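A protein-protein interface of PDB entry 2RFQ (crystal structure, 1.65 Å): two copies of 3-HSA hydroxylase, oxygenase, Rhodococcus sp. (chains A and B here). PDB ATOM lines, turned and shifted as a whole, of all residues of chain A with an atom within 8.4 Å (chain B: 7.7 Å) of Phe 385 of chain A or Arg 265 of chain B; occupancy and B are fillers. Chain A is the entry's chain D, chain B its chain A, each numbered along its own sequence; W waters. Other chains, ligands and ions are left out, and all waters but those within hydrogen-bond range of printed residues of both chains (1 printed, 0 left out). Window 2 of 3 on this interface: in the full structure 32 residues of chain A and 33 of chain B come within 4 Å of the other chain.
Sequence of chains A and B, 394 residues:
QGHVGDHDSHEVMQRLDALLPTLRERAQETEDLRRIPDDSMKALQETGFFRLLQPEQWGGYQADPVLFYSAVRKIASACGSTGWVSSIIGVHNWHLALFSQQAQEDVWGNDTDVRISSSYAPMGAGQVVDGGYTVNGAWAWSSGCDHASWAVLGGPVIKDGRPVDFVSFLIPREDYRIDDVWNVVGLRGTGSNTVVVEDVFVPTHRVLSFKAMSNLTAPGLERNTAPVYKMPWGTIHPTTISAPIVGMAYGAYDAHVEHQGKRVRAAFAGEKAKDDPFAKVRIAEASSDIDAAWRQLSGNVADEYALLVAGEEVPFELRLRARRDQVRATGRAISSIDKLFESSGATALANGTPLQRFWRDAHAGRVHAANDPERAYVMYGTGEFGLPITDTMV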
ATOM      1  N   LEU A 320      13.276  17.799 -24.305  1.00  0.00           N
ATOM      2  CA  LEU A 320      12.394  18.985 -24.254  1.00  0.00           C
ATOM      3  C   LEU A 320      13.154  20.221 -23.800  1.00  0.00           C
ATOM      4  O   LEU A 320      13.016  21.300 -24.402  1.00  0.00           O
ATOM      5  CB  LEU A 320      11.181  18.741 -23.350  1.00  0.00           C
ATOM      6  CG  LEU A 320      10.104  17.800 -23.924  1.00  0.00           C
ATOM      7  CD1 LEU A 320       9.118  17.356 -22.846  1.00  0.00           C
ATOM      8  CD2 LEU A 320       9.349  18.478 -25.045  1.00  0.00           C
ATOM      9  N   VAL A 378       6.116  26.222 -26.755  1.00  0.00           N
ATOM     10  CA  VAL A 378       4.784  25.640 -26.548  1.00  0.00           C
ATOM     11  C   VAL A 378       4.906  24.135 -26.270  1.00  0.00           C
ATOM     12  O   VAL A 378       4.268  23.612 -25.344  1.00  0.00           O
ATOM     13  CB  VAL A 378       3.833  25.944 -27.740  1.00  0.00           C
ATOM     14  CG1 VAL A 378       2.545  25.181 -27.598  1.00  0.00           C
ATOM     15  CG2 VAL A 378       3.502  27.428 -27.715  1.00  0.00           C
ATOM     16  N   MET A 379       5.756  23.449 -27.037  1.00  0.00           N
ATOM     17  CA  MET A 379       5.994  22.023 -26.794  1.00  0.00           C
ATOM     18  C   MET A 379       6.529  21.798 -25.370  1.00  0.00           C
ATOM     19  O   MET A 379       6.037  20.924 -24.625  1.00  0.00           O
ATOM     20  CB  MET A 379       6.981  21.451 -27.814  1.00  0.00           C
ATOM     21  CG  MET A 379       7.172  19.983 -27.596  1.00  0.00           C
ATOM     22  SD  MET A 379       8.418  19.244 -28.894  1.00  0.00           S
ATOM     23  CE  MET A 379       9.916  20.429 -28.499  1.00  0.00           C
ATOM     24  N   TYR A 380       7.508  22.604 -24.977  1.00  0.00           N
ATOM     25  CA  TYR A 380       8.095  22.457 -23.649  1.00  0.00           C
ATOM     26  C   TYR A 380       7.009  22.591 -22.555  1.00  0.00           C
ATOM     27  O   TYR A 380       6.895  21.747 -21.646  1.00  0.00           O
ATOM     28  CB  TYR A 380       9.207  23.492 -23.418  1.00  0.00           C
ATOM     29  CG  TYR A 380       9.713  23.430 -22.004  1.00  0.00           C
ATOM     30  CD1 TYR A 380      10.662  22.477 -21.606  1.00  0.00           C
ATOM     31  CD2 TYR A 380       9.180  24.282 -21.037  1.00  0.00           C
ATOM     32  CE1 TYR A 380      11.085  22.394 -20.272  1.00  0.00           C
ATOM     33  CE2 TYR A 380       9.599  24.218 -19.703  1.00  0.00           C
ATOM     34  CZ  TYR A 380      10.551  23.288 -19.335  1.00  0.00           C
ATOM     35  OH  TYR A 380      10.957  23.227 -18.019  1.00  0.00           O
ATOM     36  N   GLY A 381       6.184  23.630 -22.678  1.00  0.00           N
ATOM     37  CA  GLY A 381       5.070  23.832 -21.726  1.00  0.00           C
ATOM     38  C   GLY A 381       4.061  22.696 -21.670  1.00  0.00           C
ATOM     39  O   GLY A 381       3.644  22.274 -20.590  1.00  0.00           O
ATOM     40  N   THR A 382       3.677  22.190 -22.847  1.00  0.00           N
ATOM     41  CA  THR A 382       2.799  21.032 -22.960  1.00  0.00           C
ATOM     42  C   THR A 382       3.378  19.871 -22.149  1.00  0.00           C
ATOM     43  O   THR A 382       2.669  19.215 -21.384  1.00  0.00           O
ATOM     44  CB  THR A 382       2.674  20.641 -24.437  1.00  0.00           C
ATOM     45  OG1 THR A 382       2.097  21.744 -25.139  1.00  0.00           O
ATOM     46  CG2 THR A 382       1.800  19.393 -24.621  1.00  0.00           C
ATOM     47  N   GLY A 383       4.671  19.622 -22.341  1.00  0.00           N
ATOM     48  CA  GLY A 383       5.395  18.612 -21.554  1.00  0.00           C
ATOM     49  C   GLY A 383       5.329  18.835 -20.048  1.00  0.00           C
ATOM     50  O   GLY A 383       5.070  17.899 -19.284  1.00  0.00           O
ATOM     51  N   GLU A 384       5.546  20.071 -19.610  1.00  0.00           N
ATOM     52  CA  GLU A 384       5.480  20.390 -18.180  1.00  0.00           C
ATOM     53  C   GLU A 384       4.121  20.112 -17.546  1.00  0.00           C
ATOM     54  O   GLU A 384       4.035  19.831 -16.343  1.00  0.00           O
ATOM     55  CB  GLU A 384       5.855  21.847 -17.943  1.00  0.00           C
ATOM     56  CG  GLU A 384       7.336  22.159 -18.151  1.00  0.00           C
ATOM     57  CD  GLU A 384       8.230  21.409 -17.187  1.00  0.00           C
ATOM     58  OE1 GLU A 384       8.492  21.932 -16.084  1.00  0.00           O
ATOM     59  OE2 GLU A 384       8.625  20.261 -17.526  1.00  0.00           O
ATOM     60  N   PHE A 385       3.069  20.211 -18.355  1.00  0.00           N
ATOM     61  CA  PHE A 385       1.699  19.938 -17.910  1.00  0.00           C
ATOM     62  C   PHE A 385       1.311  18.458 -18.025  1.00  0.00           C
ATOM     63  O   PHE A 385       0.198  18.064 -17.613  1.00  0.00           O
ATOM     64  CB  PHE A 385       0.714  20.773 -18.725  1.00  0.00           C
ATOM     65  CG  PHE A 385       0.809  22.254 -18.493  1.00  0.00           C
ATOM     66  CD1 PHE A 385       1.283  22.768 -17.283  1.00  0.00           C
ATOM     67  CD2 PHE A 385       0.373  23.141 -19.472  1.00  0.00           C
ATOM     68  CE1 PHE A 385       1.340  24.151 -17.060  1.00  0.00           C
ATOM     69  CE2 PHE A 385       0.420  24.522 -19.266  1.00  0.00           C
ATOM     70  CZ  PHE A 385       0.902  25.030 -18.045  1.00  0.00           C
ATOM     71  N   GLY A 386       2.209  17.642 -18.573  1.00  0.00           N
ATOM     72  CA  GLY A 386       1.953  16.193 -18.765  1.00  0.00           C
ATOM     73  C   GLY A 386       0.964  15.894 -19.883  1.00  0.00           C
ATOM     74  O   GLY A 386       0.299  14.844 -19.870  1.00  0.00           O
ATOM     75  N   LEU A 387       0.849  16.799 -20.852  1.00  0.00           N
ATOM     76  CA  LEU A 387      -0.082  16.609 -21.978  1.00  0.00           C
ATOM     77  C   LEU A 387       0.629  15.950 -23.162  1.00  0.00           C
ATOM     78  O   LEU A 387       1.842  16.080 -23.305  1.00  0.00           O
ATOM     79  CB  LEU A 387      -0.687  17.937 -22.418  1.00  0.00           C
ATOM     80  CG  LEU A 387      -1.603  18.722 -21.481  1.00  0.00           C
ATOM     81  CD1 LEU A 387      -1.706  20.141 -21.983  1.00  0.00           C
ATOM     82  CD2 LEU A 387      -2.972  18.079 -21.371  1.00  0.00           C
ATOM     83  N   PRO A 388      -0.127  15.230 -24.018  1.00  0.00           N
ATOM     84  CA  PRO A 388       0.476  14.605 -25.202  1.00  0.00           C
ATOM     85  C   PRO A 388       1.195  15.590 -26.119  1.00  0.00           C
ATOM     86  O   PRO A 388       0.698  16.695 -26.397  1.00  0.00           O
ATOM     87  CB  PRO A 388      -0.732  14.003 -25.942  1.00  0.00           C
ATOM     88  CG  PRO A 388      -1.744  13.815 -24.913  1.00  0.00           C
ATOM     89  CD  PRO A 388      -1.562  14.911 -23.908  1.00  0.00           C
ATOM     90  N   ILE A 389       2.340  15.141 -26.621  1.00  0.00           N
ATOM     91  CA  ILE A 389       3.100  15.876 -27.626  1.00  0.00           C
ATOM     92  C   ILE A 389       3.164  15.069 -28.921  1.00  0.00           C
ATOM     93  O   ILE A 389       3.545  13.891 -28.892  1.00  0.00           O
ATOM     94  CB  ILE A 389       4.521  16.148 -27.105  1.00  0.00           C
ATOM     95  CG1 ILE A 389       4.470  17.216 -26.009  1.00  0.00           C
ATOM     96  CG2 ILE A 389       5.461  16.563 -28.234  1.00  0.00           C
ATOM     97  CD1 ILE A 389       5.641  17.173 -25.068  1.00  0.00           C
ATOM     98  N   TYR B 253       8.697  28.634  -9.678  1.00  0.00           N
ATOM     99  CA  TYR B 253       8.438  27.839 -10.896  1.00  0.00           C
ATOM    100  C   TYR B 253       7.702  26.526 -10.570  1.00  0.00           C
ATOM    101  O   TYR B 253       6.659  26.206 -11.166  1.00  0.00           O
ATOM    102  CB  TYR B 253       9.768  27.557 -11.598  1.00  0.00           C
ATOM    103  CG  TYR B 253       9.543  26.765 -12.855  1.00  0.00           C
ATOM    104  CD1 TYR B 253       9.161  27.403 -14.038  1.00  0.00           C
ATOM    105  CD2 TYR B 253       9.652  25.370 -12.847  1.00  0.00           C
ATOM    106  CE1 TYR B 253       8.911  26.652 -15.198  1.00  0.00           C
ATOM    107  CE2 TYR B 253       9.416  24.604 -14.024  1.00  0.00           C
ATOM    108  CZ  TYR B 253       9.036  25.267 -15.177  1.00  0.00           C
ATOM    109  OH  TYR B 253       8.804  24.528 -16.326  1.00  0.00           O
ATOM    110  N   HIS B 256       4.135  27.138  -9.361  1.00  0.00           N
ATOM    111  CA  HIS B 256       3.304  27.550 -10.500  1.00  0.00           C
ATOM    112  C   HIS B 256       2.965  26.384 -11.402  1.00  0.00           C
ATOM    113  O   HIS B 256       1.791  26.149 -11.722  1.00  0.00           O
ATOM    114  CB  HIS B 256       4.025  28.645 -11.303  1.00  0.00           C
ATOM    115  CG  HIS B 256       3.296  29.066 -12.544  1.00  0.00           C
ATOM    116  ND1 HIS B 256       2.165  29.858 -12.511  1.00  0.00           N
ATOM    117  CD2 HIS B 256       3.548  28.821 -13.854  1.00  0.00           C
ATOM    118  CE1 HIS B 256       1.758  30.087 -13.750  1.00  0.00           C
ATOM    119  NE2 HIS B 256       2.588  29.475 -14.584  1.00  0.00           N
ATOM    120  N   VAL B 257       3.977  25.613 -11.790  1.00  0.00           N
ATOM    121  CA  VAL B 257       3.718  24.463 -12.680  1.00  0.00           C
ATOM    122  C   VAL B 257       2.845  23.386 -12.016  1.00  0.00           C
ATOM    123  O   VAL B 257       1.971  22.811 -12.675  1.00  0.00           O
ATOM    124  CB  VAL B 257       5.025  23.892 -13.271  1.00  0.00           C
ATOM    125  CG1 VAL B 257       4.780  22.568 -14.059  1.00  0.00           C
ATOM    126  CG2 VAL B 257       5.684  24.938 -14.155  1.00  0.00           C
ATOM    127  N   GLU B 258       3.050  23.137 -10.719  1.00  0.00           N
ATOM    128  CA  GLU B 258       2.190  22.176  -9.998  1.00  0.00           C
ATOM    129  C   GLU B 258       0.738  22.627 -10.004  1.00  0.00           C
ATOM    130  O   GLU B 258      -0.156  21.854 -10.372  1.00  0.00           O
ATOM    131  CB  GLU B 258       2.669  21.987  -8.563  1.00  0.00           C
ATOM    132  CG  GLU B 258       1.733  21.103  -7.715  1.00  0.00           C
ATOM    133  CD  GLU B 258       2.293  20.890  -6.334  1.00  0.00           C
ATOM    134  OE1 GLU B 258       2.201  21.815  -5.501  1.00  0.00           O
ATOM    135  OE2 GLU B 258       2.846  19.798  -6.090  1.00  0.00           O
ATOM    136  N   HIS B 259       0.504  23.889  -9.656  1.00  0.00           N
ATOM    137  CA  HIS B 259      -0.858  24.404  -9.601  1.00  0.00           C
ATOM    138  C   HIS B 259      -1.492  24.453 -10.995  1.00  0.00           C
ATOM    139  O   HIS B 259      -2.618  23.975 -11.192  1.00  0.00           O
ATOM    140  CB  HIS B 259      -0.892  25.777  -8.955  1.00  0.00           C
ATOM    141  CG  HIS B 259      -2.271  26.327  -8.821  1.00  0.00           C
ATOM    142  ND1 HIS B 259      -3.120  25.949  -7.803  1.00  0.00           N
ATOM    143  CD2 HIS B 259      -2.969  27.194  -9.597  1.00  0.00           C
ATOM    144  CE1 HIS B 259      -4.273  26.582  -7.940  1.00  0.00           C
ATOM    145  NE2 HIS B 259      -4.212  27.335  -9.024  1.00  0.00           N
ATOM    146  N   GLN B 260      -0.761  25.007 -11.960  1.00  0.00           N
ATOM    147  CA  GLN B 260      -1.269  25.113 -13.326  1.00  0.00           C
ATOM    148  C   GLN B 260      -1.465  23.753 -13.980  1.00  0.00           C
ATOM    149  O   GLN B 260      -2.450  23.551 -14.690  1.00  0.00           O
ATOM    150  CB  GLN B 260      -0.368  26.002 -14.182  1.00  0.00           C
ATOM    151  CG  GLN B 260      -0.354  27.455 -13.739  1.00  0.00           C
ATOM    152  CD  GLN B 260      -1.747  28.076 -13.695  1.00  0.00           C
ATOM    153  OE1 GLN B 260      -2.617  27.729 -14.504  1.00  0.00           O
ATOM    154  NE2 GLN B 260      -1.970  28.984 -12.738  1.00  0.00           N
ATOM    155  N   GLY B 261      -0.549  22.819 -13.730  1.00  0.00           N
ATOM    156  CA  GLY B 261      -0.635  21.470 -14.312  1.00  0.00           C
ATOM    157  C   GLY B 261      -1.941  20.804 -13.942  1.00  0.00           C
ATOM    158  O   GLY B 261      -2.608  20.209 -14.787  1.00  0.00           O
ATOM    159  N   LYS B 262      -2.305  20.918 -12.669  1.00  0.00           N
ATOM    160  CA  LYS B 262      -3.574  20.407 -12.172  1.00  0.00           C
ATOM    161  C   LYS B 262      -4.751  21.064 -12.860  1.00  0.00           C
ATOM    162  O   LYS B 262      -5.664  20.372 -13.290  1.00  0.00           O
ATOM    163  CB  LYS B 262      -3.662  20.585 -10.667  1.00  0.00           C
ATOM    164  CG  LYS B 262      -2.831  19.560  -9.915  1.00  0.00           C
ATOM    165  CD  LYS B 262      -3.065  19.628  -8.426  1.00  0.00           C
ATOM    166  CE  LYS B 262      -1.974  20.413  -7.719  1.00  0.00           C
ATOM    167  NZ  LYS B 262      -1.759  19.893  -6.327  1.00  0.00           N
ATOM    168  N   ARG B 263      -4.712  22.390 -12.987  1.00  0.00           N
ATOM    169  CA  ARG B 263      -5.773  23.122 -13.673  1.00  0.00           C
ATOM    170  C   ARG B 263      -5.959  22.663 -15.115  1.00  0.00           C
ATOM    171  O   ARG B 263      -7.091  22.384 -15.537  1.00  0.00           O
ATOM    172  CB  ARG B 263      -5.490  24.617 -13.682  1.00  0.00           C
ATOM    173  CG  ARG B 263      -5.531  25.286 -12.327  1.00  0.00           C
ATOM    174  CD  ARG B 263      -5.440  26.790 -12.499  1.00  0.00           C
ATOM    175  NE  ARG B 263      -6.570  27.309 -13.270  1.00  0.00           N
ATOM    176  CZ  ARG B 263      -6.484  27.918 -14.451  1.00  0.00           C
ATOM    177  NH1 ARG B 263      -5.308  28.121 -15.025  1.00  0.00           N
ATOM    178  NH2 ARG B 263      -7.588  28.342 -15.059  1.00  0.00           N
ATOM    179  N   VAL B 264      -4.856  22.596 -15.867  1.00  0.00           N
ATOM    180  CA  VAL B 264      -4.907  22.249 -17.293  1.00  0.00           C
ATOM    181  C   VAL B 264      -5.358  20.807 -17.533  1.00  0.00           C
ATOM    182  O   VAL B 264      -6.085  20.536 -18.490  1.00  0.00           O
ATOM    183  CB  VAL B 264      -3.555  22.536 -18.024  1.00  0.00           C
ATOM    184  CG1 VAL B 264      -2.413  21.881 -17.318  1.00  0.00           C
ATOM    185  CG2 VAL B 264      -3.598  22.076 -19.491  1.00  0.00           C
ATOM    186  N   ARG B 265      -4.923  19.885 -16.673  1.00  0.00           N
ATOM    187  CA  ARG B 265      -5.272  18.478 -16.861  1.00  0.00           C
ATOM    188  C   ARG B 265      -6.723  18.261 -16.473  1.00  0.00           C
ATOM    189  O   ARG B 265      -7.402  17.431 -17.076  1.00  0.00           O
ATOM    190  CB  ARG B 265      -4.343  17.538 -16.083  1.00  0.00           C
ATOM    191  CG  ARG B 265      -2.977  17.341 -16.737  1.00  0.00           C
ATOM    192  CD  ARG B 265      -2.128  16.302 -16.000  1.00  0.00           C
ATOM    193  NE  ARG B 265      -2.036  16.579 -14.565  1.00  0.00           N
ATOM    194  CZ  ARG B 265      -1.112  17.350 -13.992  1.00  0.00           C
ATOM    195  NH1 ARG B 265      -0.178  17.946 -14.726  1.00  0.00           N
ATOM    196  NH2 ARG B 265      -1.128  17.528 -12.672  1.00  0.00           N
ATOM    197  N   ALA B 266      -7.187  19.019 -15.478  1.00  0.00           N
ATOM    198  CA  ALA B 266      -8.577  18.962 -15.012  1.00  0.00           C
ATOM    199  C   ALA B 266      -9.539  19.724 -15.917  1.00  0.00           C
ATOM    200  O   ALA B 266     -10.761  19.546 -15.825  1.00  0.00           O
ATOM    201  CB  ALA B 266      -8.685  19.484 -13.588  1.00  0.00           C
ATOM    202  N   ALA B 267      -8.991  20.584 -16.774  1.00  0.00           N
ATOM    203  CA  ALA B 267      -9.795  21.411 -17.669  1.00  0.00           C
ATOM    204  C   ALA B 267     -10.501  20.544 -18.699  1.00  0.00           C
ATOM    205  O   ALA B 267     -10.184  19.366 -18.853  1.00  0.00           O
ATOM    206  CB  ALA B 267      -8.933  22.481 -18.349  1.00  0.00           C
ATOM    207  N   PHE B 268     -11.473  21.132 -19.385  1.00  0.00           N
ATOM    208  CA  PHE B 268     -12.227  20.423 -20.399  1.00  0.00           C
ATOM    209  C   PHE B 268     -11.828  20.915 -21.777  1.00  0.00           C
ATOM    210  O   PHE B 268     -11.246  21.998 -21.923  1.00  0.00           O
ATOM    211  CB  PHE B 268     -13.732  20.613 -20.176  1.00  0.00           C
ATOM    212  CG  PHE B 268     -14.265  19.897 -18.968  1.00  0.00           C
ATOM    213  CD1 PHE B 268     -14.778  18.612 -19.079  1.00  0.00           C
ATOM    214  CD2 PHE B 268     -14.259  20.506 -17.718  1.00  0.00           C
ATOM    215  CE1 PHE B 268     -15.284  17.947 -17.967  1.00  0.00           C
ATOM    216  CE2 PHE B 268     -14.761  19.843 -16.594  1.00  0.00           C
ATOM    217  CZ  PHE B 268     -15.278  18.564 -16.722  1.00  0.00           C
ATOM    218  N   ALA B 273      -7.777  27.252 -20.353  1.00  0.00           N
ATOM    219  CA  ALA B 273      -6.679  26.603 -19.643  1.00  0.00           C
ATOM    220  C   ALA B 273      -6.164  25.359 -20.335  1.00  0.00           C
ATOM    221  O   ALA B 273      -5.023  24.967 -20.119  1.00  0.00           O
ATOM    222  CB  ALA B 273      -7.090  26.254 -18.223  1.00  0.00           C
ATOM    223  N   LYS B 274      -6.988  24.719 -21.151  1.00  0.00           N
ATOM    224  CA  LYS B 274      -6.554  23.461 -21.736  1.00  0.00           C
ATOM    225  C   LYS B 274      -5.580  23.666 -22.898  1.00  0.00           C
ATOM    226  O   LYS B 274      -4.736  22.804 -23.158  1.00  0.00           O
ATOM    227  CB  LYS B 274      -7.746  22.593 -22.150  1.00  0.00           C
ATOM    228  CG  LYS B 274      -7.361  21.213 -22.691  1.00  0.00           C
ATOM    229  CD  LYS B 274      -6.805  20.284 -21.613  1.00  0.00           C
ATOM    230  CE  LYS B 274      -7.893  19.405 -21.031  1.00  0.00           C
ATOM    231  NZ  LYS B 274      -7.404  18.539 -19.914  1.00  0.00           N
ATOM    232  N   ASP B 275      -5.703  24.795 -23.593  1.00  0.00           N
ATOM    233  CA  ASP B 275      -4.853  25.082 -24.748  1.00  0.00           C
ATOM    234  C   ASP B 275      -4.504  26.570 -24.766  1.00  0.00           C
ATOM    235  O   ASP B 275      -5.011  27.348 -25.585  1.00  0.00           O
ATOM    236  CB  ASP B 275      -5.527  24.648 -26.052  1.00  0.00           C
ATOM    237  N   ASP B 276      -3.680  26.971 -23.808  1.00  0.00           N
ATOM    238  CA  ASP B 276      -3.216  28.358 -23.737  1.00  0.00           C
ATOM    239  C   ASP B 276      -1.736  28.378 -24.106  1.00  0.00           C
ATOM    240  O   ASP B 276      -0.870  28.128 -23.258  1.00  0.00           O
ATOM    241  CB  ASP B 276      -3.430  28.909 -22.321  1.00  0.00           C
ATOM    242  CG  ASP B 276      -2.950  30.362 -22.148  1.00  0.00           C
ATOM    243  OD1 ASP B 276      -3.202  30.917 -21.070  1.00  0.00           O
ATOM    244  OD2 ASP B 276      -2.354  30.958 -23.063  1.00  0.00           O
ATOM    245  N   PRO B 277      -1.433  28.729 -25.360  1.00  0.00           N
ATOM    246  CA  PRO B 277      -0.031  28.646 -25.720  1.00  0.00           C
ATOM    247  C   PRO B 277       0.790  29.726 -25.027  1.00  0.00           C
ATOM    248  O   PRO B 277       1.996  29.561 -24.865  1.00  0.00           O
ATOM    249  CB  PRO B 277      -0.034  28.856 -27.245  1.00  0.00           C
ATOM    250  CG  PRO B 277      -1.264  29.656 -27.521  1.00  0.00           C
ATOM    251  CD  PRO B 277      -2.277  29.214 -26.473  1.00  0.00           C
ATOM    252  N   ALA B 279       0.558  30.786 -21.854  1.00  0.00           N
ATOM    253  CA  ALA B 279       0.966  30.315 -20.533  1.00  0.00           C
ATOM    254  C   ALA B 279       2.135  29.336 -20.692  1.00  0.00           C
ATOM    255  O   ALA B 279       3.094  29.352 -19.895  1.00  0.00           O
ATOM    256  CB  ALA B 279      -0.195  29.661 -19.792  1.00  0.00           C
ATOM    257  N   LYS B 280       2.063  28.504 -21.731  1.00  0.00           N
ATOM    258  CA  LYS B 280       3.142  27.548 -22.012  1.00  0.00           C
ATOM    259  C   LYS B 280       4.431  28.280 -22.336  1.00  0.00           C
ATOM    260  O   LYS B 280       5.525  27.912 -21.850  1.00  0.00           O
ATOM    261  CB  LYS B 280       2.749  26.626 -23.156  1.00  0.00           C
ATOM    262  CG  LYS B 280       1.593  25.712 -22.779  1.00  0.00           C
ATOM    263  CD  LYS B 280       1.132  24.882 -23.963  1.00  0.00           C
ATOM    264  CE  LYS B 280       0.023  23.921 -23.556  1.00  0.00           C
ATOM    265  NZ  LYS B 280      -0.427  23.148 -24.769  1.00  0.00           N
ATOM    266  N   VAL B 281       4.333  29.336 -23.149  1.00  0.00           N
ATOM    267  CA  VAL B 281       5.548  30.095 -23.496  1.00  0.00           C
ATOM    268  C   VAL B 281       6.179  30.756 -22.249  1.00  0.00           C
ATOM    269  O   VAL B 281       7.402  30.760 -22.065  1.00  0.00           O
ATOM    270  CB  VAL B 281       5.246  31.155 -24.581  1.00  0.00           C
ATOM    271  CG1 VAL B 281       6.401  32.170 -24.690  1.00  0.00           C
ATOM    272  CG2 VAL B 281       4.958  30.435 -25.900  1.00  0.00           C
ATOM    273  N   ILE B 283       6.090  29.728 -19.212  1.00  0.00           N
ATOM    274  CA  ILE B 283       6.768  28.629 -18.499  1.00  0.00           C
ATOM    275  C   ILE B 283       8.114  28.263 -19.143  1.00  0.00           C
ATOM    276  O   ILE B 283       9.107  28.026 -18.427  1.00  0.00           O
ATOM    277  CB  ILE B 283       5.809  27.414 -18.354  1.00  0.00           C
ATOM    278  CG1 ILE B 283       4.937  27.638 -17.107  1.00  0.00           C
ATOM    279  CG2 ILE B 283       6.549  26.072 -18.260  1.00  0.00           C
ATOM    280  CD1 ILE B 283       3.599  26.856 -17.180  1.00  0.00           C
ATOM    281  N   SER B 343       1.438  35.514 -15.290  1.00  0.00           N
ATOM    282  CA  SER B 343       0.659  34.455 -15.973  1.00  0.00           C
ATOM    283  C   SER B 343      -0.430  33.836 -15.083  1.00  0.00           C
ATOM    284  O   SER B 343      -1.563  33.571 -15.522  1.00  0.00           O
ATOM    285  CB  SER B 343       1.614  33.359 -16.431  1.00  0.00           C
ATOM    286  OG  SER B 343       0.925  32.420 -17.241  1.00  0.00           O
HETATM  287  O   HOH W   1       2.263  19.712 -14.252  1.00  0.00           O
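The side-chain amino group (NZ) of Lys 274 of chain B is in hydrogen-bond range of the backbone carbonyl oxygen (O) of Arg 265 of chain B.
The side-chain carboxylate (OE1) of Glu 384 of chain A lies close to the side-chain hydroxyl (OH) of Tyr 380 of chain A (3.4 Å).
The backbone carbonyl oxygen (O) of Thr 382 of chain A is in hydrogen-bond range of the backbone NH (N) of Leu 387 of chain A (3.1 Å).
O of Gly 261 of chain B is in hydrogen-bond range of NH1 of Arg 265 of chain B, at 3.3 Å.
The guanidinium group (NH1) of Arg 263 of chain B is in hydrogen-bond range of the side-chain amide oxygen (OE1) of Gln 260 of chain B (2.8 Å).
The backbone carbonyl oxygen (O) of Val 378 of chain A is in hydrogen-bond range of the side-chain hydroxyl (OG1) of Thr 382 of chain A (2.9 Å).
No position is printed for both chains.
Of the 17 pairs that touch across the chains among the printed residues, none has its exchanged pair printed and touching as well.
Printed residues of chain B within 4 Å of Gly 381 of chain A: Lys 280 (3.9 Å).
Of the printed residues of chain B, Phe 385 of chain A touches Gln 260, Gly 261, Val 264, Arg 265, Lys 280 and Ile 283.
Of the printed residues of chain B, Leu 387 of chain A touches Val 264.
Of the printed residues of chain A, Tyr 253 of chain B touches Tyr 380 and Glu 384.
Gly 261 of chain B touches just one residue of chain A: Phe 385 (3.8 Å).
Of chain A, only Phe 385 (2.9 Å) comes within 4 Å of Arg 265 of chain B.
No residue of chain A comes within 4 Å of Ala 266 of chain B.
Of the printed residues of chain A, Pro 277 of chain B touches Val 378 (3.8 Å).
The nearest printed residue of chain B that does not touch Phe 385 of chain A is Val 257 of chain B (4.6 Å).
The nearest residue of chain A that does not touch Arg 265 of chain B is Gly 386 of chain A (4.5 Å).
OH of Tyr 253 of chain B is in hydrogen-bond range of OH of Tyr 380 of chain A (3.0 Å).
The guanidinium group of Arg 265 of chain B lies within hydrogen-bond range of the backbone carbonyl oxygen of Phe 385 of chain A (2.9 Å).
The side-chain hydroxyl of Thr 382 of chain A lies within hydrogen-bond range of the side-chain amino group of Lys 280 of chain B (2.9 Å).
The side-chain hydroxyl (OH) of Tyr 253 of chain B sits at hydrogen-bond distance from the side-chain carboxylate (OE1) of Glu 384 of chain A.
Of the 24 printed residues of chain B, 10 touch a printed residue of chain A.
Hydrophobic or aromatic side chains of chain B that line the printed part of chain A: Tyr 253, Val 257, Val 264, Pro 277, Val 281 and Ile 283.
Of the 13 printed residues of chain A, 7 touch a printed residue of chain B.
Hydrophobic or aromatic side chains of chain A that line the printed part of chain B: Val 378, Tyr 380, Phe 385 and Leu 387.
Water W1 lies within hydrogen-bond range of the backbone carbonyl oxygen of Glu 384 of chain A, the guanidinium group of Arg 265 of chain B and the backbone carbonyl oxygen of Val 257 of chain B.
Among the printed residues, pairs that only touch across the chains: Phe 385 of chain A with Ile 283 of chain B (3.4 Å), Phe 385 of chain A with Val 264 of chain B (3.4 Å), Glu 384 of chain A with Val 257 of chain B (3.6 Å), Val 378 of chain A with Lys 280 of chain B (3.7 Å), Leu 387 of chain A with Val 264 of chain B (3.7 Å), Phe 385 of chain A with Gly 261 of chain B (3.8 Å), Val 378 of chain A with Val 281 of chain B (3.8 Å), Phe 385 of chain A with Gln 260 of chain B (3.8 Å), Val 378 of chain A with Pro 277 of chain B (3.8 Å), Tyr 380 of chain A with Ile 283 of chain B (3.8 Å), Phe 385 of chain A with Lys 280 of chain B (3.9 Å), Gly 381 of chain A with Lys 280 of chain B (3.9 Å) and Glu 384 of chain A with Ile 283 of chain B (3.99 Å).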
